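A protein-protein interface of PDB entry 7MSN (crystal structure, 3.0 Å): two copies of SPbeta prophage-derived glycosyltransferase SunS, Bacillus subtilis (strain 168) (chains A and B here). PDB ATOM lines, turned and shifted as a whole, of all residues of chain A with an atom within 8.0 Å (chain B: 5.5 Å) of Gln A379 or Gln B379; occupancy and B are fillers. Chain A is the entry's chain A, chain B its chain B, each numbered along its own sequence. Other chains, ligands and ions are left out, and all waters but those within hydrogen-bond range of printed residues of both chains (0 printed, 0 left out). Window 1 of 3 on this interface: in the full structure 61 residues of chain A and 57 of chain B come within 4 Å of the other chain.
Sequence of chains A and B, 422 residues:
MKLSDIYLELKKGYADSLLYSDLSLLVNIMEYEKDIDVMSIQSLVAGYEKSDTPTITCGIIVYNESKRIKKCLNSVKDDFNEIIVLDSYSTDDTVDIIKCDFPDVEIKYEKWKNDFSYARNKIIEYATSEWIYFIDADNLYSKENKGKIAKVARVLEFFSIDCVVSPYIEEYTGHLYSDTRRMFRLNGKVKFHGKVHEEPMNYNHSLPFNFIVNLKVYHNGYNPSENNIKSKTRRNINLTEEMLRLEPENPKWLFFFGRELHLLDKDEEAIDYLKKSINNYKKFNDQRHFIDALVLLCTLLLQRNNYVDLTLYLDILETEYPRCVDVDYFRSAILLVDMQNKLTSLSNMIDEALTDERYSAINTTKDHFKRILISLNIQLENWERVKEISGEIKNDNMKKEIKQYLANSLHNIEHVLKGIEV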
ATOM      1  N   LEU A 336      12.097  23.400  -1.439  1.00  0.00           N
ATOM      2  CA  LEU A 336      13.145  22.707  -0.693  1.00  0.00           C
ATOM      3  C   LEU A 336      14.484  23.433  -0.772  1.00  0.00           C
ATOM      4  O   LEU A 336      15.230  23.481   0.211  1.00  0.00           O
ATOM      5  CB  LEU A 336      13.264  21.269  -1.197  1.00  0.00           C
ATOM      6  CG  LEU A 336      14.465  20.416  -0.802  1.00  0.00           C
ATOM      7  CD1 LEU A 336      14.489  20.087   0.682  1.00  0.00           C
ATOM      8  CD2 LEU A 336      14.411  19.141  -1.635  1.00  0.00           C
ATOM      9  N   VAL A 337      14.817  24.002  -1.924  1.00  0.00           N
ATOM     10  CA  VAL A 337      16.016  24.831  -1.988  1.00  0.00           C
ATOM     11  C   VAL A 337      15.874  26.049  -1.094  1.00  0.00           C
ATOM     12  O   VAL A 337      16.831  26.446  -0.428  1.00  0.00           O
ATOM     13  CB  VAL A 337      16.337  25.215  -3.445  1.00  0.00           C
ATOM     14  CG1 VAL A 337      17.458  26.224  -3.496  1.00  0.00           C
ATOM     15  CG2 VAL A 337      16.769  23.965  -4.209  1.00  0.00           C
ATOM     16  N   MET A 339      14.413  26.146   1.650  1.00  0.00           N
ATOM     17  CA  MET A 339      14.632  25.665   3.014  1.00  0.00           C
ATOM     18  C   MET A 339      16.110  25.652   3.352  1.00  0.00           C
ATOM     19  O   MET A 339      16.547  26.238   4.346  1.00  0.00           O
ATOM     20  CB  MET A 339      14.087  24.248   3.184  1.00  0.00           C
ATOM     21  CG  MET A 339      12.591  24.038   3.044  1.00  0.00           C
ATOM     22  SD  MET A 339      11.551  24.829   4.269  1.00  0.00           S
ATOM     23  CE  MET A 339       9.996  24.400   3.490  1.00  0.00           C
ATOM     24  N   GLN A 340      16.880  24.924   2.561  1.00  0.00           N
ATOM     25  CA  GLN A 340      18.327  24.872   2.643  1.00  0.00           C
ATOM     26  C   GLN A 340      18.895  26.267   2.894  1.00  0.00           C
ATOM     27  O   GLN A 340      19.840  26.452   3.666  1.00  0.00           O
ATOM     28  CB  GLN A 340      18.863  24.350   1.319  1.00  0.00           C
ATOM     29  CG  GLN A 340      18.368  22.982   0.944  1.00  0.00           C
ATOM     30  CD  GLN A 340      18.851  21.908   1.870  1.00  0.00           C
ATOM     31  OE1 GLN A 340      19.996  21.937   2.327  1.00  0.00           O
ATOM     32  NE2 GLN A 340      17.987  20.932   2.149  1.00  0.00           N
ATOM     33  N   LEU A 343      17.995  27.530   6.366  1.00  0.00           N
ATOM     34  CA  LEU A 343      18.870  26.801   7.290  1.00  0.00           C
ATOM     35  C   LEU A 343      20.285  27.376   7.334  1.00  0.00           C
ATOM     36  O   LEU A 343      20.786  27.720   8.405  1.00  0.00           O
ATOM     37  CB  LEU A 343      18.917  25.329   6.900  1.00  0.00           C
ATOM     38  CG  LEU A 343      17.820  24.401   7.402  1.00  0.00           C
ATOM     39  CD1 LEU A 343      18.211  22.928   7.229  1.00  0.00           C
ATOM     40  CD2 LEU A 343      17.609  24.687   8.840  1.00  0.00           C
ATOM     41  N   LEU A 346      20.450  30.610   8.999  1.00  0.00           N
ATOM     42  CA  LEU A 346      20.390  30.433  10.449  1.00  0.00           C
ATOM     43  C   LEU A 346      21.715  29.937  11.007  1.00  0.00           C
ATOM     44  O   LEU A 346      22.191  30.451  12.023  1.00  0.00           O
ATOM     45  CB  LEU A 346      19.265  29.475  10.814  1.00  0.00           C
ATOM     46  CG  LEU A 346      19.058  29.148  12.287  1.00  0.00           C
ATOM     47  CD1 LEU A 346      18.342  30.263  12.992  1.00  0.00           C
ATOM     48  CD2 LEU A 346      18.218  27.887  12.363  1.00  0.00           C
ATOM     49  N   ILE A 372      23.256  22.850  18.554  1.00  0.00           N
ATOM     50  CA  ILE A 372      22.274  23.241  17.546  1.00  0.00           C
ATOM     51  C   ILE A 372      22.944  23.368  16.179  1.00  0.00           C
ATOM     52  O   ILE A 372      22.354  23.024  15.144  1.00  0.00           O
ATOM     53  CB  ILE A 372      21.562  24.549  17.954  1.00  0.00           C
ATOM     54  CG1 ILE A 372      20.701  24.363  19.205  1.00  0.00           C
ATOM     55  CG2 ILE A 372      20.627  25.014  16.850  1.00  0.00           C
ATOM     56  CD1 ILE A 372      19.740  23.150  19.196  1.00  0.00           C
ATOM     57  N   LEU A 373      24.188  23.867  16.157  1.00  0.00           N
ATOM     58  CA  LEU A 373      24.940  23.994  14.909  1.00  0.00           C
ATOM     59  C   LEU A 373      25.214  22.630  14.316  1.00  0.00           C
ATOM     60  O   LEU A 373      24.976  22.392  13.126  1.00  0.00           O
ATOM     61  CB  LEU A 373      26.259  24.691  15.168  1.00  0.00           C
ATOM     62  CG  LEU A 373      26.163  26.177  15.108  1.00  0.00           C
ATOM     63  CD1 LEU A 373      27.406  26.691  15.742  1.00  0.00           C
ATOM     64  CD2 LEU A 373      26.106  26.536  13.693  1.00  0.00           C
ATOM     65  N   ILE A 374      25.747  21.732  15.145  1.00  0.00           N
ATOM     66  CA  ILE A 374      25.987  20.360  14.742  1.00  0.00           C
ATOM     67  C   ILE A 374      24.734  19.778  14.148  1.00  0.00           C
ATOM     68  O   ILE A 374      24.766  19.087  13.128  1.00  0.00           O
ATOM     69  CB  ILE A 374      26.466  19.543  15.947  1.00  0.00           C
ATOM     70  CG1 ILE A 374      27.954  19.750  16.136  1.00  0.00           C
ATOM     71  CG2 ILE A 374      26.079  18.077  15.804  1.00  0.00           C
ATOM     72  CD1 ILE A 374      28.435  19.221  17.436  1.00  0.00           C
ATOM     73  N   SER A 375      23.605  20.090  14.743  1.00  0.00           N
ATOM     74  CA  SER A 375      22.382  19.495  14.251  1.00  0.00           C
ATOM     75  C   SER A 375      21.925  20.158  12.935  1.00  0.00           C
ATOM     76  O   SER A 375      21.419  19.454  12.054  1.00  0.00           O
ATOM     77  CB  SER A 375      21.342  19.540  15.378  1.00  0.00           C
ATOM     78  OG  SER A 375      20.116  18.950  15.004  1.00  0.00           O
ATOM     79  N   LEU A 376      22.126  21.475  12.740  1.00  0.00           N
ATOM     80  CA  LEU A 376      21.889  22.055  11.417  1.00  0.00           C
ATOM     81  C   LEU A 376      22.753  21.402  10.364  1.00  0.00           C
ATOM     82  O   LEU A 376      22.254  20.912   9.349  1.00  0.00           O
ATOM     83  CB  LEU A 376      22.149  23.550  11.370  1.00  0.00           C
ATOM     84  CG  LEU A 376      21.244  24.466  12.128  1.00  0.00           C
ATOM     85  CD1 LEU A 376      21.799  25.857  12.016  1.00  0.00           C
ATOM     86  CD2 LEU A 376      19.892  24.376  11.463  1.00  0.00           C
ATOM     87  N   ASN A 377      24.066  21.431  10.565  1.00  0.00           N
ATOM     88  CA  ASN A 377      24.953  20.941   9.531  1.00  0.00           C
ATOM     89  C   ASN A 377      24.836  19.427   9.324  1.00  0.00           C
ATOM     90  O   ASN A 377      25.189  18.947   8.253  1.00  0.00           O
ATOM     91  CB  ASN A 377      26.376  21.394   9.858  1.00  0.00           C
ATOM     92  CG  ASN A 377      26.569  22.893   9.655  1.00  0.00           C
ATOM     93  OD1 ASN A 377      26.483  23.392   8.538  1.00  0.00           O
ATOM     94  ND2 ASN A 377      26.777  23.620  10.744  1.00  0.00           N
ATOM     95  N   ILE A 378      24.330  18.654  10.284  1.00  0.00           N
ATOM     96  CA  ILE A 378      23.976  17.278   9.955  1.00  0.00           C
ATOM     97  C   ILE A 378      22.784  17.273   9.017  1.00  0.00           C
ATOM     98  O   ILE A 378      22.679  16.439   8.111  1.00  0.00           O
ATOM     99  CB  ILE A 378      23.703  16.451  11.231  1.00  0.00           C
ATOM    100  CG1 ILE A 378      24.998  16.084  11.942  1.00  0.00           C
ATOM    101  CG2 ILE A 378      22.894  15.171  10.960  1.00  0.00           C
ATOM    102  CD1 ILE A 378      24.753  15.451  13.290  1.00  0.00           C
ATOM    103  N   GLN A 379      21.858  18.190   9.223  1.00  0.00           N
ATOM    104  CA  GLN A 379      20.702  18.250   8.348  1.00  0.00           C
ATOM    105  C   GLN A 379      21.084  18.787   6.980  1.00  0.00           C
ATOM    106  O   GLN A 379      20.546  18.349   5.960  1.00  0.00           O
ATOM    107  CB  GLN A 379      19.631  19.121   8.975  1.00  0.00           C
ATOM    108  CG  GLN A 379      18.325  18.957   8.323  1.00  0.00           C
ATOM    109  CD  GLN A 379      17.268  19.859   8.874  1.00  0.00           C
ATOM    110  OE1 GLN A 379      17.546  20.766   9.645  1.00  0.00           O
ATOM    111  NE2 GLN A 379      16.056  19.672   8.420  1.00  0.00           N
ATOM    112  N   LEU A 380      21.986  19.757   6.956  1.00  0.00           N
ATOM    113  CA  LEU A 380      22.574  20.345   5.772  1.00  0.00           C
ATOM    114  C   LEU A 380      23.613  19.455   5.148  1.00  0.00           C
ATOM    115  O   LEU A 380      24.218  19.862   4.156  1.00  0.00           O
ATOM    116  CB  LEU A 380      23.268  21.653   6.116  1.00  0.00           C
ATOM    117  CG  LEU A 380      22.480  22.951   6.116  1.00  0.00           C
ATOM    118  CD1 LEU A 380      23.462  24.136   6.225  1.00  0.00           C
ATOM    119  CD2 LEU A 380      21.573  23.067   4.917  1.00  0.00           C
ATOM    120  N   GLU A 381      23.880  18.295   5.745  1.00  0.00           N
ATOM    121  CA  GLU A 381      24.891  17.337   5.267  1.00  0.00           C
ATOM    122  C   GLU A 381      26.245  17.997   5.000  1.00  0.00           C
ATOM    123  O   GLU A 381      27.024  17.545   4.162  1.00  0.00           O
ATOM    124  CB  GLU A 381      24.386  16.581   4.037  1.00  0.00           C
ATOM    125  CG  GLU A 381      23.695  15.266   4.403  1.00  0.00           C
ATOM    126  CD  GLU A 381      23.096  14.547   3.204  1.00  0.00           C
ATOM    127  OE1 GLU A 381      22.685  15.243   2.247  1.00  0.00           O
ATOM    128  OE2 GLU A 381      23.046  13.291   3.222  1.00  0.00           O
ATOM    129  N   ASN A 382      26.542  19.057   5.745  1.00  0.00           N
ATOM    130  CA  ASN A 382      27.788  19.813   5.652  1.00  0.00           C
ATOM    131  C   ASN A 382      28.859  19.188   6.550  1.00  0.00           C
ATOM    132  O   ASN A 382      29.489  19.863   7.362  1.00  0.00           O
ATOM    133  CB  ASN A 382      27.495  21.266   6.026  1.00  0.00           C
ATOM    134  CG  ASN A 382      28.538  22.237   5.538  1.00  0.00           C
ATOM    135  OD1 ASN A 382      29.752  22.023   5.705  1.00  0.00           O
ATOM    136  ND2 ASN A 382      28.067  23.336   4.927  1.00  0.00           N
ATOM    137  N   TRP A 383      29.065  17.867   6.389  1.00  0.00           N
ATOM    138  CA  TRP A 383      29.845  17.058   7.336  1.00  0.00           C
ATOM    139  C   TRP A 383      31.207  17.660   7.633  1.00  0.00           C
ATOM    140  O   TRP A 383      31.827  17.340   8.656  1.00  0.00           O
ATOM    141  CB  TRP A 383      30.055  15.646   6.788  1.00  0.00           C
ATOM    142  CG  TRP A 383      28.804  14.920   6.524  1.00  0.00           C
ATOM    143  CD1 TRP A 383      28.256  14.670   5.312  1.00  0.00           C
ATOM    144  CD2 TRP A 383      27.920  14.356   7.491  1.00  0.00           C
ATOM    145  NE1 TRP A 383      27.081  13.978   5.454  1.00  0.00           N
ATOM    146  CE2 TRP A 383      26.853  13.774   6.788  1.00  0.00           C
ATOM    147  CE3 TRP A 383      27.930  14.279   8.883  1.00  0.00           C
ATOM    148  CZ2 TRP A 383      25.805  13.125   7.428  1.00  0.00           C
ATOM    149  CZ3 TRP A 383      26.889  13.638   9.517  1.00  0.00           C
ATOM    150  CH2 TRP A 383      25.839  13.072   8.790  1.00  0.00           C
ATOM    151  N   VAL A 386      30.412  19.916  10.627  1.00  0.00           N
ATOM    152  CA  VAL A 386      30.100  19.029  11.743  1.00  0.00           C
ATOM    153  C   VAL A 386      31.377  18.526  12.388  1.00  0.00           C
ATOM    154  O   VAL A 386      31.387  18.170  13.569  1.00  0.00           O
ATOM    155  CB  VAL A 386      29.239  17.842  11.270  1.00  0.00           C
ATOM    156  CG1 VAL A 386      28.797  16.986  12.437  1.00  0.00           C
ATOM    157  CG2 VAL A 386      28.071  18.315  10.443  1.00  0.00           C
ATOM    158  N   TYR A 405      24.727   9.584  18.523  1.00  0.00           N
ATOM    159  CA  TYR A 405      23.759  10.012  17.517  1.00  0.00           C
ATOM    160  C   TYR A 405      24.225   9.658  16.112  1.00  0.00           C
ATOM    161  O   TYR A 405      23.460   9.095  15.321  1.00  0.00           O
ATOM    162  CB  TYR A 405      23.532  11.514  17.627  1.00  0.00           C
ATOM    163  CG  TYR A 405      22.615  12.048  16.569  1.00  0.00           C
ATOM    164  CD1 TYR A 405      21.250  12.112  16.784  1.00  0.00           C
ATOM    165  CD2 TYR A 405      23.110  12.501  15.359  1.00  0.00           C
ATOM    166  CE1 TYR A 405      20.400  12.602  15.819  1.00  0.00           C
ATOM    167  CE2 TYR A 405      22.268  12.992  14.387  1.00  0.00           C
ATOM    168  CZ  TYR A 405      20.916  13.042  14.622  1.00  0.00           C
ATOM    169  OH  TYR A 405      20.077  13.539  13.658  1.00  0.00           O
ATOM    170  N   LEU B 336      14.060  26.609  14.115  1.00  0.00           N
ATOM    171  CA  LEU B 336      14.410  25.309  13.609  1.00  0.00           C
ATOM    172  C   LEU B 336      13.222  24.363  13.728  1.00  0.00           C
ATOM    173  O   LEU B 336      13.077  23.435  12.929  1.00  0.00           O
ATOM    174  CB  LEU B 336      15.627  24.835  14.373  1.00  0.00           C
ATOM    175  CG  LEU B 336      16.437  23.669  13.874  1.00  0.00           C
ATOM    176  CD1 LEU B 336      17.790  23.878  14.516  1.00  0.00           C
ATOM    177  CD2 LEU B 336      15.842  22.290  14.194  1.00  0.00           C
ATOM    178  N   GLN B 340      11.246  22.448  10.589  1.00  0.00           N
ATOM    179  CA  GLN B 340      10.845  21.046  10.558  1.00  0.00           C
ATOM    180  C   GLN B 340       9.411  20.882  10.062  1.00  0.00           C
ATOM    181  O   GLN B 340       9.101  19.942   9.328  1.00  0.00           O
ATOM    182  CB  GLN B 340      11.004  20.435  11.946  1.00  0.00           C
ATOM    183  CG  GLN B 340      12.432  20.392  12.375  1.00  0.00           C
ATOM    184  CD  GLN B 340      13.347  20.029  11.226  1.00  0.00           C
ATOM    185  OE1 GLN B 340      14.193  20.827  10.820  1.00  0.00           O
ATOM    186  NE2 GLN B 340      13.234  18.794  10.739  1.00  0.00           N
ATOM    187  N   LEU B 343       9.230  21.501   6.350  1.00  0.00           N
ATOM    188  CA  LEU B 343       9.660  20.286   5.674  1.00  0.00           C
ATOM    189  C   LEU B 343       8.578  19.238   5.701  1.00  0.00           C
ATOM    190  O   LEU B 343       8.223  18.687   4.663  1.00  0.00           O
ATOM    191  CB  LEU B 343      10.951  19.734   6.273  1.00  0.00           C
ATOM    192  CG  LEU B 343      12.190  20.448   5.724  1.00  0.00           C
ATOM    193  CD1 LEU B 343      13.323  20.517   6.686  1.00  0.00           C
ATOM    194  CD2 LEU B 343      12.643  19.734   4.457  1.00  0.00           C
ATOM    195  N   ILE B 374      12.935  10.783  -0.478  1.00  0.00           N
ATOM    196  CA  ILE B 374      14.062  10.265   0.301  1.00  0.00           C
ATOM    197  C   ILE B 374      14.840  11.424   0.912  1.00  0.00           C
ATOM    198  O   ILE B 374      14.953  11.559   2.136  1.00  0.00           O
ATOM    199  CB  ILE B 374      14.984   9.399  -0.578  1.00  0.00           C
ATOM    200  CG1 ILE B 374      14.261   8.206  -1.184  1.00  0.00           C
ATOM    201  CG2 ILE B 374      16.185   8.936   0.216  1.00  0.00           C
ATOM    202  CD1 ILE B 374      13.874   7.219  -0.196  1.00  0.00           C
ATOM    203  N   SER B 375      15.382  12.279   0.047  1.00  0.00           N
ATOM    204  CA  SER B 375      16.159  13.471   0.367  1.00  0.00           C
ATOM    205  C   SER B 375      15.512  14.211   1.526  1.00  0.00           C
ATOM    206  O   SER B 375      16.183  14.625   2.479  1.00  0.00           O
ATOM    207  CB  SER B 375      16.259  14.360  -0.896  1.00  0.00           C
ATOM    208  OG  SER B 375      16.982  15.571  -0.719  1.00  0.00           O
ATOM    209  N   LEU B 376      14.193  14.320   1.462  1.00  0.00           N
ATOM    210  CA  LEU B 376      13.451  15.182   2.356  1.00  0.00           C
ATOM    211  C   LEU B 376      13.125  14.479   3.676  1.00  0.00           C
ATOM    212  O   LEU B 376      13.032  15.137   4.707  1.00  0.00           O
ATOM    213  CB  LEU B 376      12.191  15.648   1.632  1.00  0.00           C
ATOM    214  CG  LEU B 376      11.434  16.826   2.184  1.00  0.00           C
ATOM    215  CD1 LEU B 376      10.643  17.368   1.041  1.00  0.00           C
ATOM    216  CD2 LEU B 376      10.553  16.432   3.265  1.00  0.00           C
ATOM    217  N   ASN B 377      12.981  13.153   3.689  1.00  0.00           N
ATOM    218  CA  ASN B 377      12.763  12.452   4.953  1.00  0.00           C
ATOM    219  C   ASN B 377      14.065  12.001   5.616  1.00  0.00           C
ATOM    220  O   ASN B 377      14.092  11.833   6.835  1.00  0.00           O
ATOM    221  CB  ASN B 377      11.847  11.233   4.769  1.00  0.00           C
ATOM    222  CG  ASN B 377      10.404  11.606   4.508  1.00  0.00           C
ATOM    223  OD1 ASN B 377       9.568  11.612   5.405  1.00  0.00           O
ATOM    224  ND2 ASN B 377      10.089  11.842   3.259  1.00  0.00           N
ATOM    225  N   ILE B 378      15.151  11.770   4.871  1.00  0.00           N
ATOM    226  CA  ILE B 378      16.447  11.703   5.545  1.00  0.00           C
ATOM    227  C   ILE B 378      16.661  12.967   6.342  1.00  0.00           C
ATOM    228  O   ILE B 378      17.063  12.930   7.510  1.00  0.00           O
ATOM    229  CB  ILE B 378      17.605  11.496   4.554  1.00  0.00           C
ATOM    230  CG1 ILE B 378      17.561  10.132   3.891  1.00  0.00           C
ATOM    231  CG2 ILE B 378      18.933  11.721   5.235  1.00  0.00           C
ATOM    232  CD1 ILE B 378      18.565  10.035   2.760  1.00  0.00           C
ATOM    233  N   GLN B 379      16.373  14.109   5.719  1.00  0.00           N
ATOM    234  CA  GLN B 379      16.653  15.385   6.356  1.00  0.00           C
ATOM    235  C   GLN B 379      15.899  15.508   7.673  1.00  0.00           C
ATOM    236  O   GLN B 379      16.457  15.971   8.680  1.00  0.00           O
ATOM    237  CB  GLN B 379      16.279  16.503   5.405  1.00  0.00           C
ATOM    238  CG  GLN B 379      17.123  17.694   5.590  1.00  0.00           C
ATOM    239  CD  GLN B 379      16.644  18.849   4.788  1.00  0.00           C
ATOM    240  OE1 GLN B 379      16.223  18.682   3.643  1.00  0.00           O
ATOM    241  NE2 GLN B 379      16.686  20.041   5.380  1.00  0.00           N
ATOM    242  N   LEU B 380      14.641  15.040   7.686  1.00  0.00           N
ATOM    243  CA  LEU B 380      13.750  14.927   8.837  1.00  0.00           C
ATOM    244  C   LEU B 380      14.068  13.745   9.758  1.00  0.00           C
ATOM    245  O   LEU B 380      13.252  13.424  10.626  1.00  0.00           O
ATOM    246  CB  LEU B 380      12.301  14.784   8.372  1.00  0.00           C
ATOM    247  CG  LEU B 380      11.542  15.936   7.737  1.00  0.00           C
ATOM    248  CD1 LEU B 380      10.224  15.428   7.220  1.00  0.00           C
ATOM    249  CD2 LEU B 380      11.319  17.030   8.733  1.00  0.00           C
ATOM    250  N   GLU B 381      15.192  13.065   9.582  1.00  0.00           N
ATOM    251  CA  GLU B 381      15.589  11.953  10.444  1.00  0.00           C
ATOM    252  C   GLU B 381      14.537  10.832  10.460  1.00  0.00           C
ATOM    253  O   GLU B 381      14.491  10.016  11.383  1.00  0.00           O
ATOM    254  CB  GLU B 381      15.882  12.446  11.875  1.00  0.00           C
ATOM    255  CG  GLU B 381      16.918  13.563  11.939  1.00  0.00           C
ATOM    256  CD  GLU B 381      18.315  13.132  11.490  1.00  0.00           C
ATOM    257  OE1 GLU B 381      18.614  11.913  11.438  1.00  0.00           O
ATOM    258  OE2 GLU B 381      19.119  14.032  11.147  1.00  0.00           O
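Gln A379 touches just these residues of chain B: Gln B340, Leu B343 and Gln B379.
Of the printed residues of chain B, Leu A336 touches Gln B379 (3.7 Å).
Printed residues of chain B within 4 Å of Leu A343: Gln B379 (3.8 Å).
Of the printed residues of chain B, Ile A372 touches Leu B336 (3.8 Å).
Printed residues of chain A within 4 Å of Glu B381: Ile A378 (3.9 Å) and Tyr A405 (2.7 Å).
Of the printed residues of chain B, Tyr A405 touches Glu B381 (2.7 Å).
Ile B378 touches none of the printed residues of chain A.
Ile B374 touches none of the printed residues of chain A.
The nearest residue of chain A that does not touch Gln B379 is Met A339 (5.4 Å).
Hydrophobic or aromatic side chains of chain A within 4 Å of the printed part of chain B: Leu A336, Leu A343, Ile A372, Leu A376, Ile A378 and Tyr A405.
Hydrophobic or aromatic side chains of chain B that line the printed part of chain A: Leu B336 and Leu B343.
Among the printed residues, no Asp or Glu carboxylate lies within 4 Å of a Lys or Arg side-chain nitrogen of the other chain.
NE2 of Gln A340 is in hydrogen-bond range of OE1 of Gln B379, 3.2 Å away.
NE2 of Gln A379 sits at hydrogen-bond distance from OE1 of Gln B340 (3.3 Å).
The side-chain amide nitrogen (NE2) of Gln A379 lies close to the side-chain amide nitrogen (NE2) of Gln B379.
The side-chain carboxylate (OE2) of Glu B381 is in hydrogen-bond range of the side-chain hydroxyl (OH) of Tyr A405 (2.7 Å).
Among the printed residues, pairs that only touch across the chains: Gln A379 with Leu B343, Leu A336 with Gln B379, Leu A376 with Leu B336, Leu A343 with Gln B379, Ile A372 with Leu B336 and Ile A378 with Glu B381.
Leu A336 touches Gln B379, but with the chains exchanged Gln A379 does not touch Leu B336 (5.1 Å).
Gln A340 touches Gln B379, and with the chains exchanged Gln A379 touches Gln B340.
Leu A376 touches Leu B336, but with the chains exchanged Leu A336 does not touch Leu B376 (4.7 Å).
Gln A379 touches its own counterpart, Gln B379.
Positions printed for both chains: 336, 340, 343, 374, 375, 376, 377, 378, 379, 380 and 381.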
